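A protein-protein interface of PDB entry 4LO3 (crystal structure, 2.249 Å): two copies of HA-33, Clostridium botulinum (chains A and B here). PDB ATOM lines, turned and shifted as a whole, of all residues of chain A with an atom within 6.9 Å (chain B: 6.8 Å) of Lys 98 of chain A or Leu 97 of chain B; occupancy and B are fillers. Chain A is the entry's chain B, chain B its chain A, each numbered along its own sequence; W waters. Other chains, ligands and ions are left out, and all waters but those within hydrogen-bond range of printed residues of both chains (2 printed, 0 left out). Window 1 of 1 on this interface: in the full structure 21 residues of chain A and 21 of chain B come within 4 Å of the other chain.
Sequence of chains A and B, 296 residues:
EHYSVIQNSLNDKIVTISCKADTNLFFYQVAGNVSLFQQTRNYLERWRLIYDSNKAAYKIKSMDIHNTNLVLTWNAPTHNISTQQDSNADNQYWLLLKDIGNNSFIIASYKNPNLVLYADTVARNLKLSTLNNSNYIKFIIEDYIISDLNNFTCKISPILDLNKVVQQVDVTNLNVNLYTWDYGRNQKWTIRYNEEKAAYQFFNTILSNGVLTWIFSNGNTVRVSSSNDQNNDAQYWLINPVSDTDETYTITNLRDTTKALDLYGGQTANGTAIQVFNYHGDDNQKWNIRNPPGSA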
ATOM      1  N   LEU A  96       4.361  21.050   4.140  1.00  0.00           N
ATOM      2  CA  LEU A  96       5.452  21.328   3.206  1.00  0.00           C
ATOM      3  C   LEU A  96       5.955  19.981   2.717  1.00  0.00           C
ATOM      4  O   LEU A  96       6.607  19.248   3.460  1.00  0.00           O
ATOM      5  CB  LEU A  96       6.584  22.131   3.872  1.00  0.00           C
ATOM      6  CG  LEU A  96       6.169  23.530   4.386  1.00  0.00           C
ATOM      7  CD1 LEU A  96       7.353  24.328   4.946  1.00  0.00           C
ATOM      8  CD2 LEU A  96       5.455  24.359   3.323  1.00  0.00           C
ATOM      9  N   LEU A  97       5.610  19.650   1.477  1.00  0.00           N
ATOM     10  CA  LEU A  97       5.959  18.363   0.898  1.00  0.00           C
ATOM     11  C   LEU A  97       7.055  18.576  -0.128  1.00  0.00           C
ATOM     12  O   LEU A  97       6.824  19.197  -1.178  1.00  0.00           O
ATOM     13  CB  LEU A  97       4.738  17.750   0.219  1.00  0.00           C
ATOM     14  CG  LEU A  97       3.513  17.701   1.127  1.00  0.00           C
ATOM     15  CD1 LEU A  97       2.283  17.168   0.365  1.00  0.00           C
ATOM     16  CD2 LEU A  97       3.829  16.844   2.346  1.00  0.00           C
ATOM     17  N   LYS A  98       8.249  18.076   0.175  1.00  0.00           N
ATOM     18  CA  LYS A  98       9.366  18.244  -0.738  1.00  0.00           C
ATOM     19  C   LYS A  98       9.363  17.128  -1.781  1.00  0.00           C
ATOM     20  O   LYS A  98       9.437  15.945  -1.437  1.00  0.00           O
ATOM     21  CB  LYS A  98      10.694  18.251   0.016  1.00  0.00           C
ATOM     22  CG  LYS A  98      11.872  18.644  -0.858  1.00  0.00           C
ATOM     23  CD  LYS A  98      13.122  18.908  -0.027  1.00  0.00           C
ATOM     24  CE  LYS A  98      14.338  19.033  -0.935  1.00  0.00           C
ATOM     25  NZ  LYS A  98      15.330  20.028  -0.436  1.00  0.00           N
ATOM     26  N   ASP A  99       9.243  17.523  -3.046  1.00  0.00           N
ATOM     27  CA  ASP A  99       9.275  16.580  -4.159  1.00  0.00           C
ATOM     28  C   ASP A  99      10.733  16.172  -4.440  1.00  0.00           C
ATOM     29  O   ASP A  99      11.465  16.872  -5.147  1.00  0.00           O
ATOM     30  CB  ASP A  99       8.633  17.225  -5.396  1.00  0.00           C
ATOM     31  CG  ASP A  99       8.466  16.248  -6.551  1.00  0.00           C
ATOM     32  OD1 ASP A  99       8.937  15.088  -6.456  1.00  0.00           O
ATOM     33  OD2 ASP A  99       7.870  16.653  -7.573  1.00  0.00           O
ATOM     34  N   ILE A 100      11.148  15.041  -3.888  1.00  0.00           N
ATOM     35  CA  ILE A 100      12.551  14.632  -3.983  1.00  0.00           C
ATOM     36  C   ILE A 100      12.996  14.363  -5.415  1.00  0.00           C
ATOM     37  O   ILE A 100      12.268  13.757  -6.200  1.00  0.00           O
ATOM     38  CB  ILE A 100      12.857  13.382  -3.134  1.00  0.00           C
ATOM     39  CG1 ILE A 100      12.404  13.610  -1.703  1.00  0.00           C
ATOM     40  CG2 ILE A 100      14.358  13.095  -3.136  1.00  0.00           C
ATOM     41  CD1 ILE A 100      13.135  14.743  -1.034  1.00  0.00           C
ATOM     42  N   GLY A 101      14.200  14.817  -5.745  1.00  0.00           N
ATOM     43  CA  GLY A 101      14.735  14.659  -7.084  1.00  0.00           C
ATOM     44  C   GLY A 101      14.398  15.863  -7.948  1.00  0.00           C
ATOM     45  O   GLY A 101      15.120  16.190  -8.899  1.00  0.00           O
ATOM     46  N   ASN A 102      13.301  16.532  -7.603  1.00  0.00           N
ATOM     47  CA  ASN A 102      12.846  17.690  -8.349  1.00  0.00           C
ATOM     48  C   ASN A 102      13.230  18.973  -7.635  1.00  0.00           C
ATOM     49  O   ASN A 102      13.152  20.063  -8.211  1.00  0.00           O
ATOM     50  CB  ASN A 102      11.331  17.619  -8.544  1.00  0.00           C
ATOM     51  CG  ASN A 102      10.838  18.595  -9.567  1.00  0.00           C
ATOM     52  OD1 ASN A 102      10.082  19.502  -9.251  1.00  0.00           O
ATOM     53  ND2 ASN A 102      11.281  18.429 -10.808  1.00  0.00           N
ATOM     54  N   ASN A 103      13.628  18.833  -6.372  1.00  0.00           N
ATOM     55  CA  ASN A 103      14.081  19.968  -5.574  1.00  0.00           C
ATOM     56  C   ASN A 103      13.061  21.117  -5.483  1.00  0.00           C
ATOM     57  O   ASN A 103      13.423  22.298  -5.543  1.00  0.00           O
ATOM     58  CB  ASN A 103      15.407  20.500  -6.116  1.00  0.00           C
ATOM     59  CG  ASN A 103      16.316  21.007  -5.020  1.00  0.00           C
ATOM     60  OD1 ASN A 103      16.362  20.432  -3.925  1.00  0.00           O
ATOM     61  ND2 ASN A 103      17.043  22.093  -5.299  1.00  0.00           N
ATOM     62  N   SER A 104      11.788  20.759  -5.342  1.00  0.00           N
ATOM     63  CA  SER A 104      10.737  21.740  -5.176  1.00  0.00           C
ATOM     64  C   SER A 104       9.744  21.254  -4.127  1.00  0.00           C
ATOM     65  O   SER A 104       9.817  20.104  -3.648  1.00  0.00           O
ATOM     66  CB  SER A 104      10.034  22.015  -6.510  1.00  0.00           C
ATOM     67  OG  SER A 104       9.412  20.835  -6.992  1.00  0.00           O
ATOM     68  N   PHE A 105       8.822  22.144  -3.774  1.00  0.00           N
ATOM     69  CA  PHE A 105       7.866  21.886  -2.715  1.00  0.00           C
ATOM     70  C   PHE A 105       6.455  22.001  -3.229  1.00  0.00           C
ATOM     71  O   PHE A 105       6.122  22.915  -3.984  1.00  0.00           O
ATOM     72  CB  PHE A 105       8.022  22.904  -1.582  1.00  0.00           C
ATOM     73  CG  PHE A 105       9.150  22.601  -0.641  1.00  0.00           C
ATOM     74  CD1 PHE A 105       8.934  21.811   0.478  1.00  0.00           C
ATOM     75  CD2 PHE A 105      10.433  23.094  -0.882  1.00  0.00           C
ATOM     76  CE1 PHE A 105       9.977  21.520   1.354  1.00  0.00           C
ATOM     77  CE2 PHE A 105      11.486  22.808  -0.009  1.00  0.00           C
ATOM     78  CZ  PHE A 105      11.258  22.026   1.112  1.00  0.00           C
ATOM     79  N   ILE A 106       5.622  21.074  -2.793  1.00  0.00           N
ATOM     80  CA  ILE A 106       4.189  21.252  -2.895  1.00  0.00           C
ATOM     81  C   ILE A 106       3.694  21.765  -1.543  1.00  0.00           C
ATOM     82  O   ILE A 106       4.111  21.278  -0.472  1.00  0.00           O
ATOM     83  CB  ILE A 106       3.516  19.905  -3.266  1.00  0.00           C
ATOM     84  CG1 ILE A 106       3.862  19.583  -4.727  1.00  0.00           C
ATOM     85  CG2 ILE A 106       2.021  19.959  -3.037  1.00  0.00           C
ATOM     86  CD1 ILE A 106       3.523  18.184  -5.136  1.00  0.00           C
ATOM     87  N   LEU A 131      -4.105  17.967  -6.426  1.00  0.00           N
ATOM     88  CA  LEU A 131      -2.767  17.591  -6.881  1.00  0.00           C
ATOM     89  C   LEU A 131      -2.724  17.171  -8.346  1.00  0.00           C
ATOM     90  O   LEU A 131      -3.598  16.457  -8.815  1.00  0.00           O
ATOM     91  CB  LEU A 131      -2.236  16.437  -6.037  1.00  0.00           C
ATOM     92  CG  LEU A 131      -1.479  16.779  -4.772  1.00  0.00           C
ATOM     93  CD1 LEU A 131      -1.259  15.497  -3.979  1.00  0.00           C
ATOM     94  CD2 LEU A 131      -0.152  17.408  -5.158  1.00  0.00           C
ATOM     95  N   LYS A 138       4.297  23.747  -7.939  1.00  0.00           N
ATOM     96  CA  LYS A 138       5.610  23.518  -7.344  1.00  0.00           C
ATOM     97  C   LYS A 138       6.277  24.837  -7.000  1.00  0.00           C
ATOM     98  O   LYS A 138       6.137  25.832  -7.720  1.00  0.00           O
ATOM     99  CB  LYS A 138       6.491  22.658  -8.258  1.00  0.00           C
ATOM    100  CG  LYS A 138       6.007  21.209  -8.383  1.00  0.00           C
ATOM    101  CD  LYS A 138       6.847  20.455  -9.427  1.00  0.00           C
ATOM    102  CE  LYS A 138       6.477  18.963  -9.493  1.00  0.00           C
ATOM    103  NZ  LYS A 138       5.507  18.648 -10.600  1.00  0.00           N
ATOM    104  N   ILE A 141      11.600  26.883  -2.160  1.00  0.00           N
ATOM    105  CA  ILE A 141      11.693  27.491  -0.841  1.00  0.00           C
ATOM    106  C   ILE A 141      13.158  27.540  -0.467  1.00  0.00           C
ATOM    107  O   ILE A 141      13.821  26.510  -0.431  1.00  0.00           O
ATOM    108  CB  ILE A 141      10.952  26.660   0.222  1.00  0.00           C
ATOM    109  CG1 ILE A 141       9.461  26.565  -0.104  1.00  0.00           C
ATOM    110  CG2 ILE A 141      11.165  27.248   1.615  1.00  0.00           C
ATOM    111  CD1 ILE A 141       8.669  25.725   0.922  1.00  0.00           C
ATOM    112  N   LEU B  95       5.212   9.738  -7.246  1.00  0.00           N
ATOM    113  CA  LEU B  95       5.876  10.924  -6.735  1.00  0.00           C
ATOM    114  C   LEU B  95       6.215  10.685  -5.279  1.00  0.00           C
ATOM    115  O   LEU B  95       5.339  10.332  -4.491  1.00  0.00           O
ATOM    116  CB  LEU B  95       4.941  12.130  -6.826  1.00  0.00           C
ATOM    117  CG  LEU B  95       4.258  12.398  -8.163  1.00  0.00           C
ATOM    118  CD1 LEU B  95       3.390  13.680  -8.024  1.00  0.00           C
ATOM    119  CD2 LEU B  95       5.283  12.551  -9.288  1.00  0.00           C
ATOM    120  N   LEU B  96       7.482  10.848  -4.918  1.00  0.00           N
ATOM    121  CA  LEU B  96       7.890  10.701  -3.528  1.00  0.00           C
ATOM    122  C   LEU B  96       7.954  12.078  -2.894  1.00  0.00           C
ATOM    123  O   LEU B  96       8.884  12.858  -3.165  1.00  0.00           O
ATOM    124  CB  LEU B  96       9.252  10.018  -3.427  1.00  0.00           C
ATOM    125  CG  LEU B  96       9.257   8.655  -4.110  1.00  0.00           C
ATOM    126  CD1 LEU B  96      10.584   7.953  -3.840  1.00  0.00           C
ATOM    127  CD2 LEU B  96       8.101   7.798  -3.621  1.00  0.00           C
ATOM    128  N   LEU B  97       6.955  12.381  -2.065  1.00  0.00           N
ATOM    129  CA  LEU B  97       6.827  13.712  -1.464  1.00  0.00           C
ATOM    130  C   LEU B  97       7.186  13.626   0.008  1.00  0.00           C
ATOM    131  O   LEU B  97       6.457  13.035   0.808  1.00  0.00           O
ATOM    132  CB  LEU B  97       5.387  14.228  -1.617  1.00  0.00           C
ATOM    133  CG  LEU B  97       4.834  14.106  -3.043  1.00  0.00           C
ATOM    134  CD1 LEU B  97       3.329  14.436  -3.095  1.00  0.00           C
ATOM    135  CD2 LEU B  97       5.620  15.025  -3.987  1.00  0.00           C
ATOM    136  N   LYS B  98       8.319  14.208   0.370  1.00  0.00           N
ATOM    137  CA  LYS B  98       8.780  14.124   1.749  1.00  0.00           C
ATOM    138  C   LYS B  98       8.151  15.208   2.627  1.00  0.00           C
ATOM    139  O   LYS B  98       8.299  16.417   2.379  1.00  0.00           O
ATOM    140  CB  LYS B  98      10.302  14.217   1.819  1.00  0.00           C
ATOM    141  CG  LYS B  98      10.903  13.771   3.165  1.00  0.00           C
ATOM    142  CD  LYS B  98      12.426  13.977   3.184  1.00  0.00           C
ATOM    143  CE  LYS B  98      13.081  13.314   4.403  1.00  0.00           C
ATOM    144  NZ  LYS B  98      14.559  13.584   4.449  1.00  0.00           N
ATOM    145  N   ASP B  99       7.433  14.760   3.647  1.00  0.00           N
ATOM    146  CA  ASP B  99       6.783  15.668   4.585  1.00  0.00           C
ATOM    147  C   ASP B  99       7.860  16.126   5.557  1.00  0.00           C
ATOM    148  O   ASP B  99       8.192  15.411   6.505  1.00  0.00           O
ATOM    149  CB  ASP B  99       5.645  14.931   5.310  1.00  0.00           C
ATOM    150  CG  ASP B  99       4.766  15.859   6.148  1.00  0.00           C
ATOM    151  OD1 ASP B  99       5.212  16.969   6.526  1.00  0.00           O
ATOM    152  OD2 ASP B  99       3.616  15.466   6.443  1.00  0.00           O
ATOM    153  N   ILE B 100       8.428  17.298   5.293  1.00  0.00           N
ATOM    154  CA  ILE B 100       9.532  17.830   6.103  1.00  0.00           C
ATOM    155  C   ILE B 100       9.138  17.989   7.566  1.00  0.00           C
ATOM    156  O   ILE B 100       8.026  18.437   7.880  1.00  0.00           O
ATOM    157  CB  ILE B 100      10.023  19.192   5.572  1.00  0.00           C
ATOM    158  CG1 ILE B 100      10.426  19.046   4.113  1.00  0.00           C
ATOM    159  CG2 ILE B 100      11.225  19.689   6.374  1.00  0.00           C
ATOM    160  CD1 ILE B 100      11.352  17.860   3.865  1.00  0.00           C
ATOM    161  N   SER B 104       8.678  11.516   6.950  1.00  0.00           N
ATOM    162  CA  SER B 104       7.838  10.527   6.297  1.00  0.00           C
ATOM    163  C   SER B 104       7.532  10.971   4.871  1.00  0.00           C
ATOM    164  O   SER B 104       7.796  12.118   4.503  1.00  0.00           O
ATOM    165  CB  SER B 104       6.559  10.281   7.095  1.00  0.00           C
ATOM    166  OG  SER B 104       5.729  11.428   7.109  1.00  0.00           O
ATOM    167  N   PHE B 105       7.008  10.049   4.069  1.00  0.00           N
ATOM    168  CA  PHE B 105       6.741  10.318   2.668  1.00  0.00           C
ATOM    169  C   PHE B 105       5.277  10.052   2.387  1.00  0.00           C
ATOM    170  O   PHE B 105       4.707   9.073   2.866  1.00  0.00           O
ATOM    171  CB  PHE B 105       7.557   9.391   1.756  1.00  0.00           C
ATOM    172  CG  PHE B 105       9.016   9.762   1.634  1.00  0.00           C
ATOM    173  CD1 PHE B 105       9.485  10.412   0.497  1.00  0.00           C
ATOM    174  CD2 PHE B 105       9.918   9.431   2.634  1.00  0.00           C
ATOM    175  CE1 PHE B 105      10.831  10.737   0.362  1.00  0.00           C
ATOM    176  CE2 PHE B 105      11.290   9.762   2.515  1.00  0.00           C
ATOM    177  CZ  PHE B 105      11.740  10.413   1.380  1.00  0.00           C
ATOM    178  N   ILE B 106       4.666  10.945   1.621  1.00  0.00           N
ATOM    179  CA  ILE B 106       3.417  10.635   0.961  1.00  0.00           C
ATOM    180  C   ILE B 106       3.811  10.149  -0.422  1.00  0.00           C
ATOM    181  O   ILE B 106       4.697  10.716  -1.064  1.00  0.00           O
ATOM    182  CB  ILE B 106       2.540  11.887   0.853  1.00  0.00           C
ATOM    183  CG1 ILE B 106       2.112  12.308   2.261  1.00  0.00           C
ATOM    184  CG2 ILE B 106       1.315  11.624  -0.031  1.00  0.00           C
ATOM    185  CD1 ILE B 106       1.288  13.623   2.276  1.00  0.00           C
ATOM    186  N   ILE B 107       3.188   9.074  -0.875  1.00  0.00           N
ATOM    187  CA  ILE B 107       3.596   8.465  -2.139  1.00  0.00           C
ATOM    188  C   ILE B 107       2.418   8.561  -3.103  1.00  0.00           C
ATOM    189  O   ILE B 107       1.443   7.815  -2.986  1.00  0.00           O
ATOM    190  CB  ILE B 107       4.000   6.990  -1.930  1.00  0.00           C
ATOM    191  CG1 ILE B 107       5.240   6.917  -1.020  1.00  0.00           C
ATOM    192  CG2 ILE B 107       4.309   6.305  -3.278  1.00  0.00           C
ATOM    193  CD1 ILE B 107       5.596   5.475  -0.603  1.00  0.00           C
ATOM    194  N   ALA B 108       2.502   9.494  -4.045  1.00  0.00           N
ATOM    195  CA  ALA B 108       1.353   9.815  -4.877  1.00  0.00           C
ATOM    196  C   ALA B 108       1.482   9.179  -6.250  1.00  0.00           C
ATOM    197  O   ALA B 108       2.589   9.069  -6.793  1.00  0.00           O
ATOM    198  CB  ALA B 108       1.199  11.343  -5.005  1.00  0.00           C
ATOM    199  N   PRO B 113      -2.151  12.135  -9.508  1.00  0.00           N
ATOM    200  CA  PRO B 113      -1.662  12.607  -8.201  1.00  0.00           C
ATOM    201  C   PRO B 113      -2.785  12.980  -7.225  1.00  0.00           C
ATOM    202  O   PRO B 113      -2.470  13.235  -6.055  1.00  0.00           O
ATOM    203  CB  PRO B 113      -0.793  13.828  -8.553  1.00  0.00           C
ATOM    204  CG  PRO B 113      -0.462  13.635 -10.030  1.00  0.00           C
ATOM    205  CD  PRO B 113      -1.682  12.981 -10.619  1.00  0.00           C
ATOM    206  N   VAL B 116      -3.062   8.753  -3.534  1.00  0.00           N
ATOM    207  CA  VAL B 116      -1.813   8.410  -2.853  1.00  0.00           C
ATOM    208  C   VAL B 116      -1.968   7.057  -2.186  1.00  0.00           C
ATOM    209  O   VAL B 116      -3.092   6.612  -1.936  1.00  0.00           O
ATOM    210  CB  VAL B 116      -1.437   9.466  -1.768  1.00  0.00           C
ATOM    211  CG1 VAL B 116      -1.372  10.859  -2.375  1.00  0.00           C
ATOM    212  CG2 VAL B 116      -2.465   9.459  -0.614  1.00  0.00           C
ATOM    213  N   LEU B 131      -6.371  12.420  -0.198  1.00  0.00           N
ATOM    214  CA  LEU B 131      -5.516  12.774   0.935  1.00  0.00           C
ATOM    215  C   LEU B 131      -6.269  13.124   2.217  1.00  0.00           C
ATOM    216  O   LEU B 131      -7.453  13.501   2.202  1.00  0.00           O
ATOM    217  CB  LEU B 131      -4.580  13.920   0.565  1.00  0.00           C
ATOM    218  CG  LEU B 131      -3.531  13.548  -0.478  1.00  0.00           C
ATOM    219  CD1 LEU B 131      -4.093  13.699  -1.876  1.00  0.00           C
ATOM    220  CD2 LEU B 131      -2.263  14.392  -0.298  1.00  0.00           C
HETATM  221  O   HOH W   1       4.728  19.531   6.658  1.00  0.00           O
HETATM  222  O   HOH W   2       8.875  12.482  -6.971  1.00  0.00           O
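N of Lys 98 of chain B is in hydrogen-bond range of O of Lys 98 of chain A, 2.7 Å away.
The backbone carbonyl oxygen (O) of Leu 96 of chain A sits close to the backbone carbonyl oxygen (O) of Lys 98 of chain B, 3.5 Å away.
O of Leu 96 of chain B lies within hydrogen-bond range of N of Ile 100 of chain A, 3.2 Å away.
The backbone NH (N) of Ile 100 of chain B lies within hydrogen-bond range of the backbone carbonyl oxygen (O) of Leu 96 of chain A, 3.2 Å away.
O of Ser 104 of chain B is in hydrogen-bond range of N of Asp 99 of chain B (2.8 Å).
The backbone NH (N) of Ile 106 of chain B sits at hydrogen-bond distance from the backbone carbonyl oxygen (O) of Leu 97 of chain B.
The backbone carbonyl oxygen of Leu 97 of chain A lies within hydrogen-bond range of the backbone NH of Ile 106 of chain A (2.8 Å).
O of Ser 104 of chain A sits at hydrogen-bond distance from N of Asp 99 of chain A (2.7 Å).
Asp 99 of chain B touches Leu 96 of chain A (CA to O, 3.8 Å).
Asp 99 of chain B touches Leu 97 of chain A (CA to CD2, 3.9 Å).
Leu 96 of chain B touches Lys 98 of chain A (O to O, 3.6 Å).
CA of Leu 97 of chain B touches O of Lys 98 of chain A, 3.4 Å away.
Leu 96 of chain B touches Asp 99 of chain A (O to CA, 3.9 Å).
CG1 of Ile 100 of chain A touches CE1 of Phe 105 of chain B (3.9 Å).
CE1 of Phe 105 of chain A touches CG1 of Ile 100 of chain B, 3.7 Å away.
Leu 97 of chain B touches Ile 106 of chain A (CD2 to CD1, 3.96 Å).
Leu 131 of chain A touches Pro 113 of chain B (CB to O, 3.2 Å).
Leu 131 of chain A touches Leu 131 of chain B.
Of the printed residues of chain B, Lys 98 of chain A touches Leu 96 (3.6 Å), Leu 97 (3.4 Å), Lys 98 (2.7 Å) and Ile 100 (3.9 Å).
Leu 97 of chain B touches three residues of chain A.
Of the printed residues of chain B, Ile 106 of chain A touches Leu 97 (3.96 Å).
Printed residues of chain B within 4 Å of Leu 97 of chain A: Lys 98 (3.4 Å) and Asp 99 (3.9 Å).
Printed residues of chain A within 4 Å of Leu 96 of chain B: Lys 98 (3.6 Å), Asp 99 (3.9 Å) and Ile 100 (3.2 Å).
Of the printed residues of chain A, Ile 100 of chain B touches Leu 96, Lys 98 and Phe 105.
Of the printed residues of chain B, Asp 99 of chain A touches Leu 96 and Leu 97.
Gly 101 of chain A touches none of the printed residues of chain B.
The nearest residue of chain B that does not touch Lys 98 of chain A is Asp 99 of chain B (4.9 Å).
The nearest residue of chain A that does not touch Leu 97 of chain B is Leu 97 of chain A (4.02 Å).
Hydrophobic or aromatic side chains of chain A within 4 Å of the printed part of chain B: Leu 97, Ile 100, Phe 105, Ile 106 and Leu 131.
Of the 14 printed residues of chain B, 8 touch a printed residue of chain A.
Among the printed residues, 17 pairs touch across the chains.
Leu 96 of chain A touches Asp 99 of chain B, and with the chains exchanged Asp 99 of chain A touches Leu 96 of chain B.
Leu 96 of chain A touches Ile 100 of chain B, and with the chains exchanged Ile 100 of chain A touches Leu 96 of chain B.
Lys 98 of chain B touches its own counterpart, Lys 98 of chain A.
Leu 131 of chain B touches its own counterpart, Leu 131 of chain A.
9 positions are printed for both chains.
Water W1 lies within hydrogen-bond range of OD1 of Asp 99 of chain B (2.6 Å) and N of Leu 96 of chain A (3.0 Å).
Water W2 bridges OD1 of Asp 99 of chain A and N of Leu 96 of chain B.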
